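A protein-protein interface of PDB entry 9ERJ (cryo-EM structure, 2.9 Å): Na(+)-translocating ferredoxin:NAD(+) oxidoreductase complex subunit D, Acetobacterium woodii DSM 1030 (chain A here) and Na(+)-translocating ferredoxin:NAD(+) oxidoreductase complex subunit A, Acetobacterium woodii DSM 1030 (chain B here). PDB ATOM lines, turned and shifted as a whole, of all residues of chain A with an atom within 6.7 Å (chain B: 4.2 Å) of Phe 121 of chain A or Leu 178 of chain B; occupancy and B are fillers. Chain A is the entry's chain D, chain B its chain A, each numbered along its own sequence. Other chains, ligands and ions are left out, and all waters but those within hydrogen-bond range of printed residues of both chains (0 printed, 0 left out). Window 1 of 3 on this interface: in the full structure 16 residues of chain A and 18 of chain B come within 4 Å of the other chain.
Ile 109 of chain A touches none of the printed residues of chain B.
Printed residues of chain B within 4 Å of Gly 118 of chain A: Arg 156.
Of the printed residues of chain B, Asn 120 of chain A touches Arg 156 (3.3 Å).
Of chain B, only Arg 156 (3.8 Å), Thr 175 (3.6 Å) and Leu 178 (3.9 Å) come within 4 Å of Phe 121 of chain A.
Of the printed residues of chain B, Ala 251 of chain A touches Arg 156 (3.0 Å).
Of the printed residues of chain A, Arg 156 of chain B touches Gly 118, Asn 120, Phe 121 and Ala 251.
Printed residues of chain A within 4 Å of Thr 175 of chain B: Phe 121 (3.6 Å).
Of chain A, only Phe 121 comes within 4 Å of Leu 178 of chain B.
The nearest residue of chain A that does not touch Leu 178 of chain B is Ile 122 of chain A (4.1 Å).
Of the 10 printed residues of chain B, 3 touch a printed residue of chain A.
Printed residues of chain B that touch a printed residue of chain A: Arg 156, Thr 175 and Leu 178.
Hydrophobic or aromatic side chains of chain A that line the printed part of chain B: Phe 121.
Among the printed residues, 6 pairs touch across the chains.
Among the printed residues, pairs that only touch across the chains: Phe 121 of chain A with Thr 175 of chain B (3.6 Å), Gly 118 of chain A with Arg 156 of chain B (3.7 Å), Phe 121 of chain A with Arg 156 of chain B (3.8 Å) and Phe 121 of chain A with Leu 178 of chain B (3.9 Å).
The guanidinium group of Arg 156 of chain B sits at hydrogen-bond distance from the backbone carbonyl oxygen of Asn 120 of chain A, 3.3 Å away.
The backbone carbonyl oxygen (O) of Ala 251 of chain A lies within hydrogen-bond range of the guanidinium group (NH1) of Arg 156 of chain B (3.0 Å).
The side-chain amide nitrogen of Asn 120 of chain A sits at hydrogen-bond distance from the backbone carbonyl oxygen of Ile 122 of chain A (3.4 Å).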
ATOM      1  N   PHE A 105      20.149 -23.786  -4.566  1.00  0.00           N
ATOM      2  CA  PHE A 105      20.599 -22.424  -4.284  1.00  0.00           C
ATOM      3  C   PHE A 105      21.124 -21.737  -5.540  1.00  0.00           C
ATOM      4  O   PHE A 105      20.874 -20.545  -5.752  1.00  0.00           O
ATOM      5  CB  PHE A 105      21.673 -22.435  -3.195  1.00  0.00           C
ATOM      6  CG  PHE A 105      22.100 -21.063  -2.746  1.00  0.00           C
ATOM      7  CD1 PHE A 105      21.415 -20.409  -1.736  1.00  0.00           C
ATOM      8  CD2 PHE A 105      23.190 -20.432  -3.323  1.00  0.00           C
ATOM      9  CE1 PHE A 105      21.803 -19.149  -1.319  1.00  0.00           C
ATOM     10  CE2 PHE A 105      23.581 -19.173  -2.911  1.00  0.00           C
ATOM     11  CZ  PHE A 105      22.887 -18.534  -1.907  1.00  0.00           C
ATOM     12  N   ILE A 109      17.910 -19.015  -6.537  1.00  0.00           N
ATOM     13  CA  ILE A 109      18.165 -17.716  -5.916  1.00  0.00           C
ATOM     14  C   ILE A 109      19.046 -16.835  -6.791  1.00  0.00           C
ATOM     15  O   ILE A 109      18.699 -15.687  -7.080  1.00  0.00           O
ATOM     16  CB  ILE A 109      18.780 -17.915  -4.514  1.00  0.00           C
ATOM     17  CG1 ILE A 109      17.708 -18.370  -3.525  1.00  0.00           C
ATOM     18  CG2 ILE A 109      19.433 -16.632  -4.022  1.00  0.00           C
ATOM     19  CD1 ILE A 109      18.227 -18.609  -2.130  1.00  0.00           C
ATOM     20  N   VAL A 110      20.202 -17.345  -7.218  1.00  0.00           N
ATOM     21  CA  VAL A 110      21.154 -16.513  -7.950  1.00  0.00           C
ATOM     22  C   VAL A 110      20.635 -16.190  -9.347  1.00  0.00           C
ATOM     23  O   VAL A 110      20.695 -15.039  -9.795  1.00  0.00           O
ATOM     24  CB  VAL A 110      22.531 -17.200  -7.997  1.00  0.00           C
ATOM     25  CG1 VAL A 110      23.423 -16.536  -9.022  1.00  0.00           C
ATOM     26  CG2 VAL A 110      23.184 -17.169  -6.627  1.00  0.00           C
ATOM     27  N   PHE A 114      16.729 -12.906 -10.629  1.00  0.00           N
ATOM     28  CA  PHE A 114      17.144 -11.703 -11.334  1.00  0.00           C
ATOM     29  C   PHE A 114      16.586 -11.619 -12.747  1.00  0.00           C
ATOM     30  O   PHE A 114      16.887 -10.658 -13.459  1.00  0.00           O
ATOM     31  CB  PHE A 114      18.672 -11.617 -11.377  1.00  0.00           C
ATOM     32  CG  PHE A 114      19.293 -11.199 -10.074  1.00  0.00           C
ATOM     33  CD1 PHE A 114      19.483 -12.117  -9.056  1.00  0.00           C
ATOM     34  CD2 PHE A 114      19.687  -9.889  -9.869  1.00  0.00           C
ATOM     35  CE1 PHE A 114      20.051 -11.735  -7.857  1.00  0.00           C
ATOM     36  CE2 PHE A 114      20.256  -9.503  -8.674  1.00  0.00           C
ATOM     37  CZ  PHE A 114      20.438 -10.427  -7.667  1.00  0.00           C
ATOM     38  N   GLY A 118      21.384 -14.951 -18.447  1.00  0.00           N
ATOM     39  CA  GLY A 118      22.102 -13.768 -18.874  1.00  0.00           C
ATOM     40  C   GLY A 118      21.727 -12.486 -18.170  1.00  0.00           C
ATOM     41  O   GLY A 118      22.167 -11.415 -18.596  1.00  0.00           O
ATOM     42  N   GLN A 119      20.932 -12.555 -17.102  1.00  0.00           N
ATOM     43  CA  GLN A 119      20.450 -11.359 -16.420  1.00  0.00           C
ATOM     44  C   GLN A 119      20.953 -11.241 -14.987  1.00  0.00           C
ATOM     45  O   GLN A 119      20.502 -10.353 -14.258  1.00  0.00           O
ATOM     46  CB  GLN A 119      18.921 -11.318 -16.448  1.00  0.00           C
ATOM     47  CG  GLN A 119      18.375 -10.498 -17.600  1.00  0.00           C
ATOM     48  CD  GLN A 119      17.283 -11.207 -18.359  1.00  0.00           C
ATOM     49  OE1 GLN A 119      16.568 -12.039 -17.806  1.00  0.00           O
ATOM     50  NE2 GLN A 119      17.154 -10.889 -19.639  1.00  0.00           N
ATOM     51  N   ASN A 120      21.868 -12.104 -14.564  1.00  0.00           N
ATOM     52  CA  ASN A 120      22.513 -11.982 -13.267  1.00  0.00           C
ATOM     53  C   ASN A 120      23.867 -11.294 -13.418  1.00  0.00           C
ATOM     54  O   ASN A 120      24.405 -11.156 -14.517  1.00  0.00           O
ATOM     55  CB  ASN A 120      22.674 -13.356 -12.611  1.00  0.00           C
ATOM     56  CG  ASN A 120      23.259 -14.386 -13.552  1.00  0.00           C
ATOM     57  OD1 ASN A 120      23.400 -14.143 -14.747  1.00  0.00           O
ATOM     58  ND2 ASN A 120      23.615 -15.543 -13.012  1.00  0.00           N
ATOM     59  N   PHE A 121      24.416 -10.857 -12.287  1.00  0.00           N
ATOM     60  CA  PHE A 121      25.704 -10.177 -12.264  1.00  0.00           C
ATOM     61  C   PHE A 121      26.788 -10.970 -11.548  1.00  0.00           C
ATOM     62  O   PHE A 121      27.919 -10.489 -11.445  1.00  0.00           O
ATOM     63  CB  PHE A 121      25.559  -8.790 -11.620  1.00  0.00           C
ATOM     64  CG  PHE A 121      25.382  -8.822 -10.124  1.00  0.00           C
ATOM     65  CD1 PHE A 121      24.146  -9.099  -9.565  1.00  0.00           C
ATOM     66  CD2 PHE A 121      26.448  -8.556  -9.277  1.00  0.00           C
ATOM     67  CE1 PHE A 121      23.978  -9.126  -8.196  1.00  0.00           C
ATOM     68  CE2 PHE A 121      26.285  -8.585  -7.906  1.00  0.00           C
ATOM     69  CZ  PHE A 121      25.050  -8.869  -7.365  1.00  0.00           C
ATOM     70  N   ILE A 122      26.479 -12.171 -11.058  1.00  0.00           N
ATOM     71  CA  ILE A 122      27.400 -12.951 -10.244  1.00  0.00           C
ATOM     72  C   ILE A 122      27.443 -14.379 -10.778  1.00  0.00           C
ATOM     73  O   ILE A 122      26.559 -14.819 -11.517  1.00  0.00           O
ATOM     74  CB  ILE A 122      27.002 -12.926  -8.746  1.00  0.00           C
ATOM     75  CG1 ILE A 122      28.235 -12.991  -7.843  1.00  0.00           C
ATOM     76  CG2 ILE A 122      26.024 -14.036  -8.415  1.00  0.00           C
ATOM     77  CD1 ILE A 122      28.855 -11.646  -7.562  1.00  0.00           C
ATOM     78  N   ASN A 123      28.501 -15.095 -10.410  1.00  0.00           N
ATOM     79  CA  ASN A 123      28.683 -16.474 -10.851  1.00  0.00           C
ATOM     80  C   ASN A 123      27.864 -17.411  -9.969  1.00  0.00           C
ATOM     81  O   ASN A 123      28.058 -17.421  -8.749  1.00  0.00           O
ATOM     82  CB  ASN A 123      30.158 -16.853 -10.797  1.00  0.00           C
ATOM     83  CG  ASN A 123      30.497 -18.026 -11.693  1.00  0.00           C
ATOM     84  OD1 ASN A 123      29.616 -18.686 -12.234  1.00  0.00           O
ATOM     85  ND2 ASN A 123      31.786 -18.287 -11.857  1.00  0.00           N
ATOM     86  N   ALA A 127      29.162 -18.970  -6.207  1.00  0.00           N
ATOM     87  CA  ALA A 127      28.394 -18.516  -5.053  1.00  0.00           C
ATOM     88  C   ALA A 127      27.781 -19.683  -4.290  1.00  0.00           C
ATOM     89  O   ALA A 127      27.765 -19.672  -3.053  1.00  0.00           O
ATOM     90  CB  ALA A 127      27.308 -17.538  -5.494  1.00  0.00           C
ATOM     91  N   ALA A 251      27.921 -13.639 -18.671  1.00  0.00           N
ATOM     92  CA  ALA A 251      27.093 -12.638 -18.011  1.00  0.00           C
ATOM     93  C   ALA A 251      27.808 -11.908 -16.881  1.00  0.00           C
ATOM     94  O   ALA A 251      27.198 -11.038 -16.252  1.00  0.00           O
ATOM     95  CB  ALA A 251      25.819 -13.289 -17.468  1.00  0.00           C
ATOM     96  N   SER A 252      29.072 -12.233 -16.606  1.00  0.00           N
ATOM     97  CA  SER A 252      29.808 -11.608 -15.516  1.00  0.00           C
ATOM     98  C   SER A 252      31.109 -10.941 -15.940  1.00  0.00           C
ATOM     99  O   SER A 252      31.777 -10.349 -15.087  1.00  0.00           O
ATOM    100  CB  SER A 252      30.119 -12.640 -14.423  1.00  0.00           C
ATOM    101  OG  SER A 252      29.047 -13.554 -14.273  1.00  0.00           O
ATOM    102  N   LEU A 289      34.924 -13.918  -7.576  1.00  0.00           N
ATOM    103  CA  LEU A 289      33.685 -13.314  -7.104  1.00  0.00           C
ATOM    104  C   LEU A 289      33.819 -11.834  -6.772  1.00  0.00           C
ATOM    105  O   LEU A 289      32.838 -11.097  -6.903  1.00  0.00           O
ATOM    106  CB  LEU A 289      33.169 -14.051  -5.865  1.00  0.00           C
ATOM    107  CG  LEU A 289      32.465 -15.394  -6.058  1.00  0.00           C
ATOM    108  CD1 LEU A 289      32.136 -16.005  -4.709  1.00  0.00           C
ATOM    109  CD2 LEU A 289      31.212 -15.229  -6.892  1.00  0.00           C
ATOM    110  N   ASN A 292      33.569  -9.751 -10.040  1.00  0.00           N
ATOM    111  CA  ASN A 292      32.224  -9.651 -10.587  1.00  0.00           C
ATOM    112  C   ASN A 292      31.471  -8.449 -10.042  1.00  0.00           C
ATOM    113  O   ASN A 292      30.503  -8.005 -10.665  1.00  0.00           O
ATOM    114  CB  ASN A 292      31.430 -10.926 -10.283  1.00  0.00           C
ATOM    115  CG  ASN A 292      31.920 -12.118 -11.068  1.00  0.00           C
ATOM    116  OD1 ASN A 292      32.734 -11.983 -11.979  1.00  0.00           O
ATOM    117  ND2 ASN A 292      31.432 -13.298 -10.716  1.00  0.00           N
ATOM    118  N   VAL A 293      31.899  -7.920  -8.897  1.00  0.00           N
ATOM    119  CA  VAL A 293      31.309  -6.721  -8.315  1.00  0.00           C
ATOM    120  C   VAL A 293      31.863  -5.446  -8.942  1.00  0.00           C
ATOM    121  O   VAL A 293      31.094  -4.503  -9.182  1.00  0.00           O
ATOM    122  CB  VAL A 293      31.523  -6.716  -6.786  1.00  0.00           C
ATOM    123  CG1 VAL A 293      31.023  -5.430  -6.158  1.00  0.00           C
ATOM    124  CG2 VAL A 293      30.842  -7.919  -6.152  1.00  0.00           C
ATOM    125  N   THR A 295      33.050  -5.137 -11.958  1.00  0.00           N
ATOM    126  CA  THR A 295      32.867  -5.174 -13.407  1.00  0.00           C
ATOM    127  C   THR A 295      32.021  -4.011 -13.935  1.00  0.00           C
ATOM    128  O   THR A 295      32.415  -3.403 -14.940  1.00  0.00           O
ATOM    129  CB  THR A 295      32.280  -6.528 -13.830  1.00  0.00           C
ATOM    130  OG1 THR A 295      33.292  -7.538 -13.733  1.00  0.00           O
ATOM    131  CG2 THR A 295      31.765  -6.483 -15.257  1.00  0.00           C
ATOM    132  N   PRO A 296      30.881  -3.643 -13.325  1.00  0.00           N
ATOM    133  CA  PRO A 296      30.156  -2.458 -13.818  1.00  0.00           C
ATOM    134  C   PRO A 296      30.923  -1.149 -13.675  1.00  0.00           C
ATOM    135  O   PRO A 296      30.571  -0.177 -14.354  1.00  0.00           O
ATOM    136  CB  PRO A 296      28.883  -2.448 -12.963  1.00  0.00           C
ATOM    137  CG  PRO A 296      28.677  -3.866 -12.628  1.00  0.00           C
ATOM    138  CD  PRO A 296      30.060  -4.339 -12.314  1.00  0.00           C
ATOM    139  N   ARG B 156      23.204  -1.707 -13.877  1.00  0.00           N
ATOM    140  CA  ARG B 156      23.156  -2.968 -14.610  1.00  0.00           C
ATOM    141  C   ARG B 156      21.908  -3.759 -14.247  1.00  0.00           C
ATOM    142  O   ARG B 156      21.329  -4.443 -15.098  1.00  0.00           O
ATOM    143  CB  ARG B 156      24.418  -3.791 -14.339  1.00  0.00           C
ATOM    144  CG  ARG B 156      24.717  -4.844 -15.404  1.00  0.00           C
ATOM    145  CD  ARG B 156      24.130  -6.197 -15.027  1.00  0.00           C
ATOM    146  NE  ARG B 156      24.036  -7.114 -16.156  1.00  0.00           N
ATOM    147  CZ  ARG B 156      24.859  -8.132 -16.367  1.00  0.00           C
ATOM    148  NH1 ARG B 156      25.876  -8.378 -15.560  1.00  0.00           N
ATOM    149  NH2 ARG B 156      24.654  -8.925 -17.413  1.00  0.00           N
ATOM    150  N   LEU B 174      18.971  -8.573  -1.704  1.00  0.00           N
ATOM    151  CA  LEU B 174      19.639  -9.756  -2.248  1.00  0.00           C
ATOM    152  C   LEU B 174      21.016  -9.414  -2.816  1.00  0.00           C
ATOM    153  O   LEU B 174      21.984 -10.167  -2.621  1.00  0.00           O
ATOM    154  CB  LEU B 174      18.760 -10.411  -3.314  1.00  0.00           C
ATOM    155  CG  LEU B 174      17.441 -11.029  -2.842  1.00  0.00           C
ATOM    156  CD1 LEU B 174      16.408 -11.012  -3.955  1.00  0.00           C
ATOM    157  CD2 LEU B 174      17.650 -12.445  -2.340  1.00  0.00           C
ATOM    158  N   THR B 175      21.125  -8.281  -3.517  1.00  0.00           N
ATOM    159  CA  THR B 175      22.422  -7.828  -4.011  1.00  0.00           C
ATOM    160  C   THR B 175      23.388  -7.559  -2.863  1.00  0.00           C
ATOM    161  O   THR B 175      24.572  -7.914  -2.941  1.00  0.00           O
ATOM    162  CB  THR B 175      22.243  -6.570  -4.860  1.00  0.00           C
ATOM    163  OG1 THR B 175      21.276  -6.815  -5.888  1.00  0.00           O
ATOM    164  CG2 THR B 175      23.556  -6.163  -5.493  1.00  0.00           C
ATOM    165  N   ALA B 176      22.897  -6.931  -1.790  1.00  0.00           N
ATOM    166  CA  ALA B 176      23.740  -6.676  -0.628  1.00  0.00           C
ATOM    167  C   ALA B 176      24.213  -7.975   0.009  1.00  0.00           C
ATOM    168  O   ALA B 176      25.355  -8.067   0.467  1.00  0.00           O
ATOM    169  CB  ALA B 176      22.987  -5.818   0.387  1.00  0.00           C
ATOM    170  N   GLY B 177      23.352  -8.995   0.042  1.00  0.00           N
ATOM    171  CA  GLY B 177      23.772 -10.287   0.570  1.00  0.00           C
ATOM    172  C   GLY B 177      24.853 -10.948  -0.268  1.00  0.00           C
ATOM    173  O   GLY B 177      25.806 -11.529   0.268  1.00  0.00           O
ATOM    174  N   LEU B 178      24.723 -10.875  -1.595  1.00  0.00           N
ATOM    175  CA  LEU B 178      25.757 -11.445  -2.460  1.00  0.00           C
ATOM    176  C   LEU B 178      27.087 -10.704  -2.307  1.00  0.00           C
ATOM    177  O   LEU B 178      28.157 -11.332  -2.255  1.00  0.00           O
ATOM    178  CB  LEU B 178      25.291 -11.438  -3.915  1.00  0.00           C
ATOM    179  CG  LEU B 178      24.036 -12.264  -4.223  1.00  0.00           C
ATOM    180  CD1 LEU B 178      23.644 -12.129  -5.684  1.00  0.00           C
ATOM    181  CD2 LEU B 178      24.234 -13.725  -3.854  1.00  0.00           C
ATOM    182  N   MET B 179      27.042  -9.369  -2.219  1.00  0.00           N
ATOM    183  CA  MET B 179      28.260  -8.608  -1.945  1.00  0.00           C
ATOM    184  C   MET B 179      28.839  -8.943  -0.575  1.00  0.00           C
ATOM    185  O   MET B 179      30.064  -8.958  -0.404  1.00  0.00           O
ATOM    186  CB  MET B 179      27.989  -7.107  -2.046  1.00  0.00           C
ATOM    187  CG  MET B 179      27.470  -6.645  -3.393  1.00  0.00           C
ATOM    188  SD  MET B 179      27.042  -4.895  -3.405  1.00  0.00           S
ATOM    189  CE  MET B 179      28.600  -4.160  -2.924  1.00  0.00           C
ATOM    190  N   ALA B 180      27.977  -9.215   0.408  1.00  0.00           N
ATOM    191  CA  ALA B 180      28.448  -9.611   1.728  1.00  0.00           C
ATOM    192  C   ALA B 180      29.173 -10.948   1.692  1.00  0.00           C
ATOM    193  O   ALA B 180      30.153 -11.131   2.414  1.00  0.00           O
ATOM    194  CB  ALA B 180      27.278  -9.665   2.709  1.00  0.00           C
ATOM    195  N   ILE B 181      28.712 -11.891   0.868  1.00  0.00           N
ATOM    196  CA  ILE B 181      29.464 -13.136   0.689  1.00  0.00           C
ATOM    197  C   ILE B 181      30.819 -12.861   0.036  1.00  0.00           C
ATOM    198  O   ILE B 181      31.871 -13.346   0.498  1.00  0.00           O
ATOM    199  CB  ILE B 181      28.643 -14.147  -0.132  1.00  0.00           C
ATOM    200  CG1 ILE B 181      27.343 -14.503   0.591  1.00  0.00           C
ATOM    201  CG2 ILE B 181      29.461 -15.396  -0.414  1.00  0.00           C
ATOM    202  CD1 ILE B 181      26.555 -15.609  -0.077  1.00  0.00           C
ATOM    203  N   ALA B 182      30.816 -12.064  -1.039  1.00  0.00           N
ATOM    204  CA  ALA B 182      32.057 -11.761  -1.751  1.00  0.00           C
ATOM    205  C   ALA B 182      33.078 -11.096  -0.833  1.00  0.00           C
ATOM    206  O   ALA B 182      34.288 -11.290  -0.988  1.00  0.00           O
ATOM    207  CB  ALA B 182      31.764 -10.879  -2.964  1.00  0.00           C
